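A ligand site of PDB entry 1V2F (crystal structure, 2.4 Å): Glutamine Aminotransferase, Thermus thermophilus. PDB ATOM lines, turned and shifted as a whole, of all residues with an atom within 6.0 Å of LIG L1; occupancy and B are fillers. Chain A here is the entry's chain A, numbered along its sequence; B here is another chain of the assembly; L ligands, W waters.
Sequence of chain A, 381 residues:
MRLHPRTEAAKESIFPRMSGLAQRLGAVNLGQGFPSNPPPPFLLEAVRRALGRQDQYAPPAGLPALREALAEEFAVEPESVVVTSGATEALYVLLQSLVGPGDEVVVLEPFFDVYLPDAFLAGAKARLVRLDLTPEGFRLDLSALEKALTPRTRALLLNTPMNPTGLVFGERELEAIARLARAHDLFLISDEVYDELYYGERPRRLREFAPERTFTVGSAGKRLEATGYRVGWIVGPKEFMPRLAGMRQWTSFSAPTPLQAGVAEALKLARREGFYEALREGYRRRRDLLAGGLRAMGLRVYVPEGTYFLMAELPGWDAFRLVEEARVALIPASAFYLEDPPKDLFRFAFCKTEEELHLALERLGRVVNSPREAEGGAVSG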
ATOM      1  N   SER A  13      -5.713 -39.087 -30.091  1.00  0.00           N
ATOM      2  CA  SER A  13      -5.971 -38.360 -28.857  1.00  0.00           C
ATOM      3  C   SER A  13      -7.481 -38.220 -28.607  1.00  0.00           C
ATOM      4  O   SER A  13      -8.241 -38.009 -29.550  1.00  0.00           O
ATOM      5  CB  SER A  13      -5.317 -36.980 -28.918  1.00  0.00           C
ATOM      6  OG  SER A  13      -5.675 -36.180 -27.807  1.00  0.00           O
ATOM      7  N   PHE A  15      -8.988 -35.821 -27.259  1.00  0.00           N
ATOM      8  CA  PHE A  15      -9.423 -34.443 -27.455  1.00  0.00           C
ATOM      9  C   PHE A  15     -10.005 -34.173 -28.848  1.00  0.00           C
ATOM     10  O   PHE A  15     -11.130 -33.709 -28.950  1.00  0.00           O
ATOM     11  CB  PHE A  15      -8.272 -33.491 -27.101  1.00  0.00           C
ATOM     12  CG  PHE A  15      -7.888 -33.556 -25.645  1.00  0.00           C
ATOM     13  CD1 PHE A  15      -8.597 -32.837 -24.689  1.00  0.00           C
ATOM     14  CD2 PHE A  15      -6.876 -34.407 -25.214  1.00  0.00           C
ATOM     15  CE1 PHE A  15      -8.330 -32.981 -23.329  1.00  0.00           C
ATOM     16  CE2 PHE A  15      -6.585 -34.554 -23.852  1.00  0.00           C
ATOM     17  CZ  PHE A  15      -7.313 -33.837 -22.912  1.00  0.00           C
ATOM     18  N   PRO A  16      -9.255 -34.447 -29.925  1.00  0.00           N
ATOM     19  CA  PRO A  16      -9.860 -34.188 -31.235  1.00  0.00           C
ATOM     20  C   PRO A  16     -10.973 -35.196 -31.561  1.00  0.00           C
ATOM     21  O   PRO A  16     -11.887 -34.891 -32.342  1.00  0.00           O
ATOM     22  CB  PRO A  16      -8.678 -34.271 -32.191  1.00  0.00           C
ATOM     23  CG  PRO A  16      -7.708 -35.168 -31.478  1.00  0.00           C
ATOM     24  CD  PRO A  16      -7.812 -34.692 -30.049  1.00  0.00           C
ATOM     25  N   GLY A  31     -15.276 -29.611 -24.673  1.00  0.00           N
ATOM     26  CA  GLY A  31     -14.168 -30.514 -24.427  1.00  0.00           C
ATOM     27  C   GLY A  31     -12.822 -29.939 -24.812  1.00  0.00           C
ATOM     28  O   GLY A  31     -12.247 -29.156 -24.055  1.00  0.00           O
ATOM     29  N   GLN A  32     -12.309 -30.332 -25.976  1.00  0.00           N
ATOM     30  CA  GLN A  32     -11.025 -29.834 -26.461  1.00  0.00           C
ATOM     31  C   GLN A  32     -10.987 -28.302 -26.353  1.00  0.00           C
ATOM     32  O   GLN A  32     -11.958 -27.624 -26.669  1.00  0.00           O
ATOM     33  CB  GLN A  32     -10.800 -30.266 -27.916  1.00  0.00           C
ATOM     34  CG  GLN A  32      -9.530 -29.711 -28.533  1.00  0.00           C
ATOM     35  CD  GLN A  32      -9.282 -30.256 -29.929  1.00  0.00           C
ATOM     36  OE1 GLN A  32     -10.218 -30.639 -30.625  1.00  0.00           O
ATOM     37  NE2 GLN A  32      -8.024 -30.276 -30.331  1.00  0.00           N
ATOM     38  N   GLY A  33      -9.845 -27.764 -25.925  1.00  0.00           N
ATOM     39  CA  GLY A  33      -9.734 -26.339 -25.748  1.00  0.00           C
ATOM     40  C   GLY A  33      -9.321 -25.437 -26.905  1.00  0.00           C
ATOM     41  O   GLY A  33      -8.152 -25.342 -27.257  1.00  0.00           O
ATOM     42  N   PHE A  34     -10.312 -24.761 -27.494  1.00  0.00           N
ATOM     43  CA  PHE A  34     -10.069 -23.795 -28.565  1.00  0.00           C
ATOM     44  C   PHE A  34     -11.257 -22.842 -28.595  1.00  0.00           C
ATOM     45  O   PHE A  34     -12.412 -23.258 -28.485  1.00  0.00           O
ATOM     46  CB  PHE A  34      -9.858 -24.483 -29.928  1.00  0.00           C
ATOM     47  CG  PHE A  34     -11.093 -25.137 -30.492  1.00  0.00           C
ATOM     48  CD1 PHE A  34     -12.030 -24.396 -31.214  1.00  0.00           C
ATOM     49  CD2 PHE A  34     -11.305 -26.514 -30.325  1.00  0.00           C
ATOM     50  CE1 PHE A  34     -13.144 -25.008 -31.763  1.00  0.00           C
ATOM     51  CE2 PHE A  34     -12.410 -27.126 -30.879  1.00  0.00           C
ATOM     52  CZ  PHE A  34     -13.337 -26.371 -31.602  1.00  0.00           C
ATOM     53  N   THR A  88       3.368 -27.603 -28.606  1.00  0.00           N
ATOM     54  CA  THR A  88       3.360 -29.058 -28.739  1.00  0.00           C
ATOM     55  C   THR A  88       4.731 -29.537 -29.181  1.00  0.00           C
ATOM     56  O   THR A  88       5.273 -30.486 -28.615  1.00  0.00           O
ATOM     57  CB  THR A  88       2.276 -29.551 -29.741  1.00  0.00           C
ATOM     58  OG1 THR A  88       0.986 -29.383 -29.158  1.00  0.00           O
ATOM     59  CG2 THR A  88       2.468 -31.028 -30.054  1.00  0.00           C
ATOM     60  N   PHE A 112      -1.230 -33.064 -18.802  1.00  0.00           N
ATOM     61  CA  PHE A 112      -1.646 -32.592 -20.112  1.00  0.00           C
ATOM     62  C   PHE A 112      -1.417 -33.755 -21.094  1.00  0.00           C
ATOM     63  O   PHE A 112      -0.500 -34.543 -20.926  1.00  0.00           O
ATOM     64  CB  PHE A 112      -0.835 -31.340 -20.521  1.00  0.00           C
ATOM     65  CG  PHE A 112      -1.171 -30.818 -21.890  1.00  0.00           C
ATOM     66  CD1 PHE A 112      -0.227 -30.850 -22.911  1.00  0.00           C
ATOM     67  CD2 PHE A 112      -2.467 -30.394 -22.188  1.00  0.00           C
ATOM     68  CE1 PHE A 112      -0.566 -30.464 -24.206  1.00  0.00           C
ATOM     69  CE2 PHE A 112      -2.815 -30.009 -23.478  1.00  0.00           C
ATOM     70  CZ  PHE A 112      -1.860 -30.049 -24.499  1.00  0.00           C
ATOM     71  N   ASP A 113      -2.272 -33.828 -22.118  1.00  0.00           N
ATOM     72  CA  ASP A 113      -2.253 -34.905 -23.110  1.00  0.00           C
ATOM     73  C   ASP A 113      -0.931 -35.392 -23.728  1.00  0.00           C
ATOM     74  O   ASP A 113      -0.788 -36.586 -23.975  1.00  0.00           O
ATOM     75  CB  ASP A 113      -3.227 -34.544 -24.257  1.00  0.00           C
ATOM     76  CG  ASP A 113      -3.556 -35.733 -25.142  1.00  0.00           C
ATOM     77  OD1 ASP A 113      -4.005 -36.771 -24.616  1.00  0.00           O
ATOM     78  OD2 ASP A 113      -3.382 -35.622 -26.373  1.00  0.00           O
ATOM     79  N   VAL A 114       0.030 -34.500 -23.974  1.00  0.00           N
ATOM     80  CA  VAL A 114       1.282 -34.927 -24.619  1.00  0.00           C
ATOM     81  C   VAL A 114       2.465 -35.316 -23.717  1.00  0.00           C
ATOM     82  O   VAL A 114       3.456 -35.873 -24.197  1.00  0.00           O
ATOM     83  CB  VAL A 114       1.806 -33.840 -25.601  1.00  0.00           C
ATOM     84  CG1 VAL A 114       0.673 -33.359 -26.509  1.00  0.00           C
ATOM     85  CG2 VAL A 114       2.423 -32.675 -24.836  1.00  0.00           C
ATOM     86  N   ASN A 163      -3.310 -27.032 -16.669  1.00  0.00           N
ATOM     87  CA  ASN A 163      -4.392 -27.650 -17.437  1.00  0.00           C
ATOM     88  C   ASN A 163      -4.352 -29.106 -16.964  1.00  0.00           C
ATOM     89  O   ASN A 163      -3.322 -29.766 -17.115  1.00  0.00           O
ATOM     90  CB  ASN A 163      -4.062 -27.556 -18.931  1.00  0.00           C
ATOM     91  CG  ASN A 163      -5.068 -28.269 -19.794  1.00  0.00           C
ATOM     92  OD1 ASN A 163      -6.027 -28.866 -19.298  1.00  0.00           O
ATOM     93  ND2 ASN A 163      -4.861 -28.204 -21.116  1.00  0.00           N
ATOM     94  N   TYR A 194      -0.566 -20.672 -20.772  1.00  0.00           N
ATOM     95  CA  TYR A 194      -1.609 -19.814 -20.210  1.00  0.00           C
ATOM     96  C   TYR A 194      -1.022 -18.765 -19.292  1.00  0.00           C
ATOM     97  O   TYR A 194      -1.705 -18.280 -18.383  1.00  0.00           O
ATOM     98  CB  TYR A 194      -2.623 -20.649 -19.419  1.00  0.00           C
ATOM     99  CG  TYR A 194      -3.491 -21.532 -20.285  1.00  0.00           C
ATOM    100  CD1 TYR A 194      -4.478 -20.980 -21.107  1.00  0.00           C
ATOM    101  CD2 TYR A 194      -3.271 -22.900 -20.346  1.00  0.00           C
ATOM    102  CE1 TYR A 194      -5.227 -21.777 -21.959  1.00  0.00           C
ATOM    103  CE2 TYR A 194      -4.022 -23.711 -21.202  1.00  0.00           C
ATOM    104  CZ  TYR A 194      -4.990 -23.135 -22.009  1.00  0.00           C
ATOM    105  OH  TYR A 194      -5.704 -23.919 -22.901  1.00  0.00           O
ATOM    106  N   LYS A 222      -2.400 -19.903 -27.681  1.00  0.00           N
ATOM    107  CA  LYS A 222      -3.078 -19.803 -26.389  1.00  0.00           C
ATOM    108  C   LYS A 222      -2.992 -18.380 -25.850  1.00  0.00           C
ATOM    109  O   LYS A 222      -3.684 -18.037 -24.898  1.00  0.00           O
ATOM    110  CB  LYS A 222      -2.474 -20.798 -25.387  1.00  0.00           C
ATOM    111  CG  LYS A 222      -2.714 -22.279 -25.746  1.00  0.00           C
ATOM    112  CD  LYS A 222      -4.205 -22.644 -25.716  1.00  0.00           C
ATOM    113  CE  LYS A 222      -4.454 -24.126 -26.071  1.00  0.00           C
ATOM    114  NZ  LYS A 222      -3.557 -24.926 -25.214  1.00  0.00           N
ATOM    115  N   PHE A 309     -10.249 -23.568 -18.295  1.00  0.00           N
ATOM    116  CA  PHE A 309     -10.825 -24.859 -17.957  1.00  0.00           C
ATOM    117  C   PHE A 309     -11.238 -24.886 -16.489  1.00  0.00           C
ATOM    118  O   PHE A 309     -10.670 -24.164 -15.663  1.00  0.00           O
ATOM    119  CB  PHE A 309      -9.812 -25.996 -18.158  1.00  0.00           C
ATOM    120  CG  PHE A 309      -9.317 -26.156 -19.563  1.00  0.00           C
ATOM    121  CD1 PHE A 309     -10.165 -26.595 -20.566  1.00  0.00           C
ATOM    122  CD2 PHE A 309      -7.997 -25.875 -19.878  1.00  0.00           C
ATOM    123  CE1 PHE A 309      -9.706 -26.762 -21.870  1.00  0.00           C
ATOM    124  CE2 PHE A 309      -7.513 -26.032 -21.176  1.00  0.00           C
ATOM    125  CZ  PHE A 309      -8.373 -26.476 -22.182  1.00  0.00           C
ATOM    126  N   PHE A 336      -6.795 -37.499 -18.051  1.00  0.00           N
ATOM    127  CA  PHE A 336      -5.666 -36.824 -17.407  1.00  0.00           C
ATOM    128  C   PHE A 336      -4.987 -37.675 -16.341  1.00  0.00           C
ATOM    129  O   PHE A 336      -3.942 -37.294 -15.804  1.00  0.00           O
ATOM    130  CB  PHE A 336      -6.156 -35.522 -16.765  1.00  0.00           C
ATOM    131  CG  PHE A 336      -7.053 -34.709 -17.644  1.00  0.00           C
ATOM    132  CD1 PHE A 336      -6.521 -33.812 -18.574  1.00  0.00           C
ATOM    133  CD2 PHE A 336      -8.438 -34.830 -17.551  1.00  0.00           C
ATOM    134  CE1 PHE A 336      -7.350 -33.052 -19.390  1.00  0.00           C
ATOM    135  CE2 PHE A 336      -9.279 -34.075 -18.370  1.00  0.00           C
ATOM    136  CZ  PHE A 336      -8.732 -33.182 -19.293  1.00  0.00           C
ATOM    137  N   ARG A 347     -13.840 -32.340 -17.069  1.00  0.00           N
ATOM    138  CA  ARG A 347     -13.241 -31.034 -17.364  1.00  0.00           C
ATOM    139  C   ARG A 347     -14.166 -30.278 -18.321  1.00  0.00           C
ATOM    140  O   ARG A 347     -14.649 -30.846 -19.300  1.00  0.00           O
ATOM    141  CB  ARG A 347     -11.865 -31.179 -18.019  1.00  0.00           C
ATOM    142  CG  ARG A 347     -11.103 -29.855 -18.113  1.00  0.00           C
ATOM    143  CD  ARG A 347      -9.868 -29.941 -18.990  1.00  0.00           C
ATOM    144  NE  ARG A 347     -10.208 -29.972 -20.408  1.00  0.00           N
ATOM    145  CZ  ARG A 347      -9.325 -29.969 -21.394  1.00  0.00           C
ATOM    146  NH1 ARG A 347      -8.027 -29.932 -21.117  1.00  0.00           N
ATOM    147  NH2 ARG A 347      -9.728 -29.974 -22.653  1.00  0.00           N
ATOM    148  N   TYR B  57      -7.564 -25.108 -34.028  1.00  0.00           N
ATOM    149  CA  TYR B  57      -7.055 -26.451 -34.293  1.00  0.00           C
ATOM    150  C   TYR B  57      -7.794 -27.223 -35.359  1.00  0.00           C
ATOM    151  O   TYR B  57      -9.021 -27.297 -35.353  1.00  0.00           O
ATOM    152  CB  TYR B  57      -7.111 -27.331 -33.037  1.00  0.00           C
ATOM    153  CG  TYR B  57      -6.169 -26.983 -31.922  1.00  0.00           C
ATOM    154  CD1 TYR B  57      -4.780 -27.005 -32.120  1.00  0.00           C
ATOM    155  CD2 TYR B  57      -6.654 -26.662 -30.663  1.00  0.00           C
ATOM    156  CE1 TYR B  57      -3.910 -26.725 -31.080  1.00  0.00           C
ATOM    157  CE2 TYR B  57      -5.792 -26.383 -29.619  1.00  0.00           C
ATOM    158  CZ  TYR B  57      -4.423 -26.405 -29.832  1.00  0.00           C
ATOM    159  OH  TYR B  57      -3.594 -26.074 -28.803  1.00  0.00           O
ATOM    160  N   TRP B 250       1.923 -35.971 -31.874  1.00  0.00           N
ATOM    161  CA  TRP B 250       2.824 -35.630 -30.773  1.00  0.00           C
ATOM    162  C   TRP B 250       3.947 -34.659 -31.138  1.00  0.00           C
ATOM    163  O   TRP B 250       4.536 -34.028 -30.253  1.00  0.00           O
ATOM    164  CB  TRP B 250       3.447 -36.907 -30.196  1.00  0.00           C
ATOM    165  CG  TRP B 250       2.444 -37.954 -29.843  1.00  0.00           C
ATOM    166  CD1 TRP B 250       2.467 -39.264 -30.213  1.00  0.00           C
ATOM    167  CD2 TRP B 250       1.264 -37.778 -29.051  1.00  0.00           C
ATOM    168  NE1 TRP B 250       1.381 -39.924 -29.702  1.00  0.00           N
ATOM    169  CE2 TRP B 250       0.623 -39.036 -28.984  1.00  0.00           C
ATOM    170  CE3 TRP B 250       0.687 -36.684 -28.388  1.00  0.00           C
ATOM    171  CZ2 TRP B 250      -0.571 -39.227 -28.275  1.00  0.00           C
ATOM    172  CZ3 TRP B 250      -0.489 -36.875 -27.688  1.00  0.00           C
ATOM    173  CH2 TRP B 250      -1.116 -38.137 -27.638  1.00  0.00           C
ATOM    174  N   PHE B 253       1.206 -31.667 -33.504  1.00  0.00           N
ATOM    175  CA  PHE B 253      -0.248 -31.844 -33.417  1.00  0.00           C
ATOM    176  C   PHE B 253      -0.986 -31.749 -34.750  1.00  0.00           C
ATOM    177  O   PHE B 253      -1.600 -32.714 -35.178  1.00  0.00           O
ATOM    178  CB  PHE B 253      -0.885 -30.880 -32.422  1.00  0.00           C
ATOM    179  CG  PHE B 253      -2.304 -31.222 -32.082  1.00  0.00           C
ATOM    180  CD1 PHE B 253      -2.591 -32.305 -31.250  1.00  0.00           C
ATOM    181  CD2 PHE B 253      -3.369 -30.516 -32.639  1.00  0.00           C
ATOM    182  CE1 PHE B 253      -3.920 -32.678 -30.976  1.00  0.00           C
ATOM    183  CE2 PHE B 253      -4.691 -30.879 -32.374  1.00  0.00           C
ATOM    184  CZ  PHE B 253      -4.965 -31.958 -31.538  1.00  0.00           C
HETATM  185  C1  LIG L   1      -6.685 -29.113 -24.376  1.00  0.00           C
HETATM  186  O1  LIG L   1      -6.297 -29.426 -23.243  1.00  0.00           O
HETATM  187  O2  LIG L   1      -7.884 -29.238 -24.725  1.00  0.00           O
HETATM  188  C2  LIG L   1      -5.862 -28.064 -25.114  1.00  0.00           C
HETATM  189  C3  LIG L   1      -5.738 -28.358 -26.605  1.00  0.00           C
HETATM  190  C4  LIG L   1      -4.872 -29.567 -26.918  1.00  0.00           C
HETATM  191  C5  LIG L   1      -5.304 -30.853 -26.605  1.00  0.00           C
HETATM  192  C6  LIG L   1      -4.521 -31.972 -26.920  1.00  0.00           C
HETATM  193  C7  LIG L   1      -3.289 -31.804 -27.557  1.00  0.00           C
HETATM  194  C8  LIG L   1      -2.843 -30.535 -27.866  1.00  0.00           C
HETATM  195  C9  LIG L   1      -3.635 -29.417 -27.546  1.00  0.00           C
HETATM  196  N1  LG2 L   2       0.413 -27.301 -23.174  1.00  0.00           N
HETATM  197  C1  LG2 L   2      -0.782 -26.982 -22.619  1.00  0.00           C
HETATM  198  C2  LG2 L   2      -0.944 -27.114 -21.085  1.00  0.00           C
HETATM  199  C3  LG2 L   2      -1.829 -26.558 -23.432  1.00  0.00           C
HETATM  200  O1  LG2 L   2      -3.079 -26.231 -22.854  1.00  0.00           O
HETATM  201  C4  LG2 L   2      -1.637 -26.464 -24.803  1.00  0.00           C
HETATM  202  C5  LG2 L   2      -2.806 -25.962 -25.693  1.00  0.00           C
HETATM  203  C6  LG2 L   2      -0.368 -26.802 -25.345  1.00  0.00           C
HETATM  204  C7  LG2 L   2       0.644 -27.227 -24.514  1.00  0.00           C
HETATM  205  C8  LG2 L   2      -0.034 -26.797 -26.836  1.00  0.00           C
HETATM  206  O2  LG2 L   2       0.004 -25.523 -27.468  1.00  0.00           O
HETATM  207  P1  LG2 L   2       0.235 -25.416 -29.021  1.00  0.00           P
HETATM  208  O3  LG2 L   2       0.863 -24.100 -29.196  1.00  0.00           O
HETATM  209  O4  LG2 L   2      -1.256 -25.498 -29.493  1.00  0.00           O
HETATM  210  O5  LG2 L   2       0.950 -26.588 -29.616  1.00  0.00           O
HETATM  211  O   HOH W   1      -4.929 -32.215 -22.145  1.00  0.00           O
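The backbone NH of Gly 33 is in hydrogen-bond range of an oxygen (O2) of LIG L1 (2.7 Å).
The guanidinium group of Arg 347 is in salt-bridge range of an oxygen (O1) of LIG L1 (2.8 Å).
ND2 of Asn 163 is in hydrogen-bond range of O1 of LIG L1, at 2.8 Å.
O1 of LG2 L2 lies within hydrogen-bond range of ND2 of Asn 163 (3.2 Å).
The side-chain hydroxyl (OH) of Tyr 57 of chain B is in hydrogen-bond range of an oxygen (O4) of LG2 L2, at 2.5 Å.
NZ of Lys 222 is covalently linked to C5 of LG2 L2.
The backbone NH (N) of Thr 88 is in hydrogen-bond range of an oxygen (O5) of LG2 L2 (2.8 Å).
The side-chain hydroxyl (OG1) of Thr 88 is in hydrogen-bond range of an oxygen (O5) of LG2 L2, at 2.8 Å.
The side-chain hydroxyl of Tyr 194 sits close to an oxygen (O1) of LG2 L2 (3.5 Å).
CD1 of Phe 15 touches O2 of LIG L1, 3.7 Å away.
Gln 32 touches LIG L1 (C to O2, 3.6 Å).
CE2 of Phe 112 touches O1 of LIG L1, at 3.5 Å.
Asp 113 touches LIG L1 (OD2 to C6, 3.9 Å).
NZ of Lys 222 touches C2 of LIG L1, at 3.9 Å.
Phe 309 touches LIG L1 (CZ to O1, 3.8 Å).
Tyr 57 of chain B touches LIG L1.
CE1 of Phe 253 of chain B touches C7 of LIG L1 (3.6 Å).
Hydrophobic or aromatic side chains within 4 Å of LIG L1: Phe 15, Phe 112, Phe 309, Tyr 57 of chain B and Phe 253 of chain B.
Within 4 Å of LIG L1: Phe 15, Gln 32, Gly 33, Phe 112, Asp 113, Asn 163, Lys 222, Phe 309, Arg 347, Tyr 57 of chain B and Phe 253 of chain B.
Water W1 bridges the backbone NH (N) of Asp 113 (3.1 Å) and an oxygen (O1) of LIG L1 (3.3 Å).
The guanidinium group of Arg 347 sits at hydrogen-bond distance from the side-chain amide oxygen of Asn 163 (2.9 Å).
The backbone carbonyl oxygen (O) of Gly 31 sits at hydrogen-bond distance from the guanidinium group (NH2) of Arg 347 (3.0 Å).
The backbone NH (N) of Phe 15 lies close to the side-chain hydroxyl (OG) of Ser 13.
The side-chain hydroxyl (OG) of Ser 13 lies within hydrogen-bond range of the side-chain carboxylate (OD2) of Asp 113.
The side-chain amino group (NZ) of Lys 222 sits at hydrogen-bond distance from the side-chain hydroxyl (OH) of Tyr 194 (3.3 Å).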
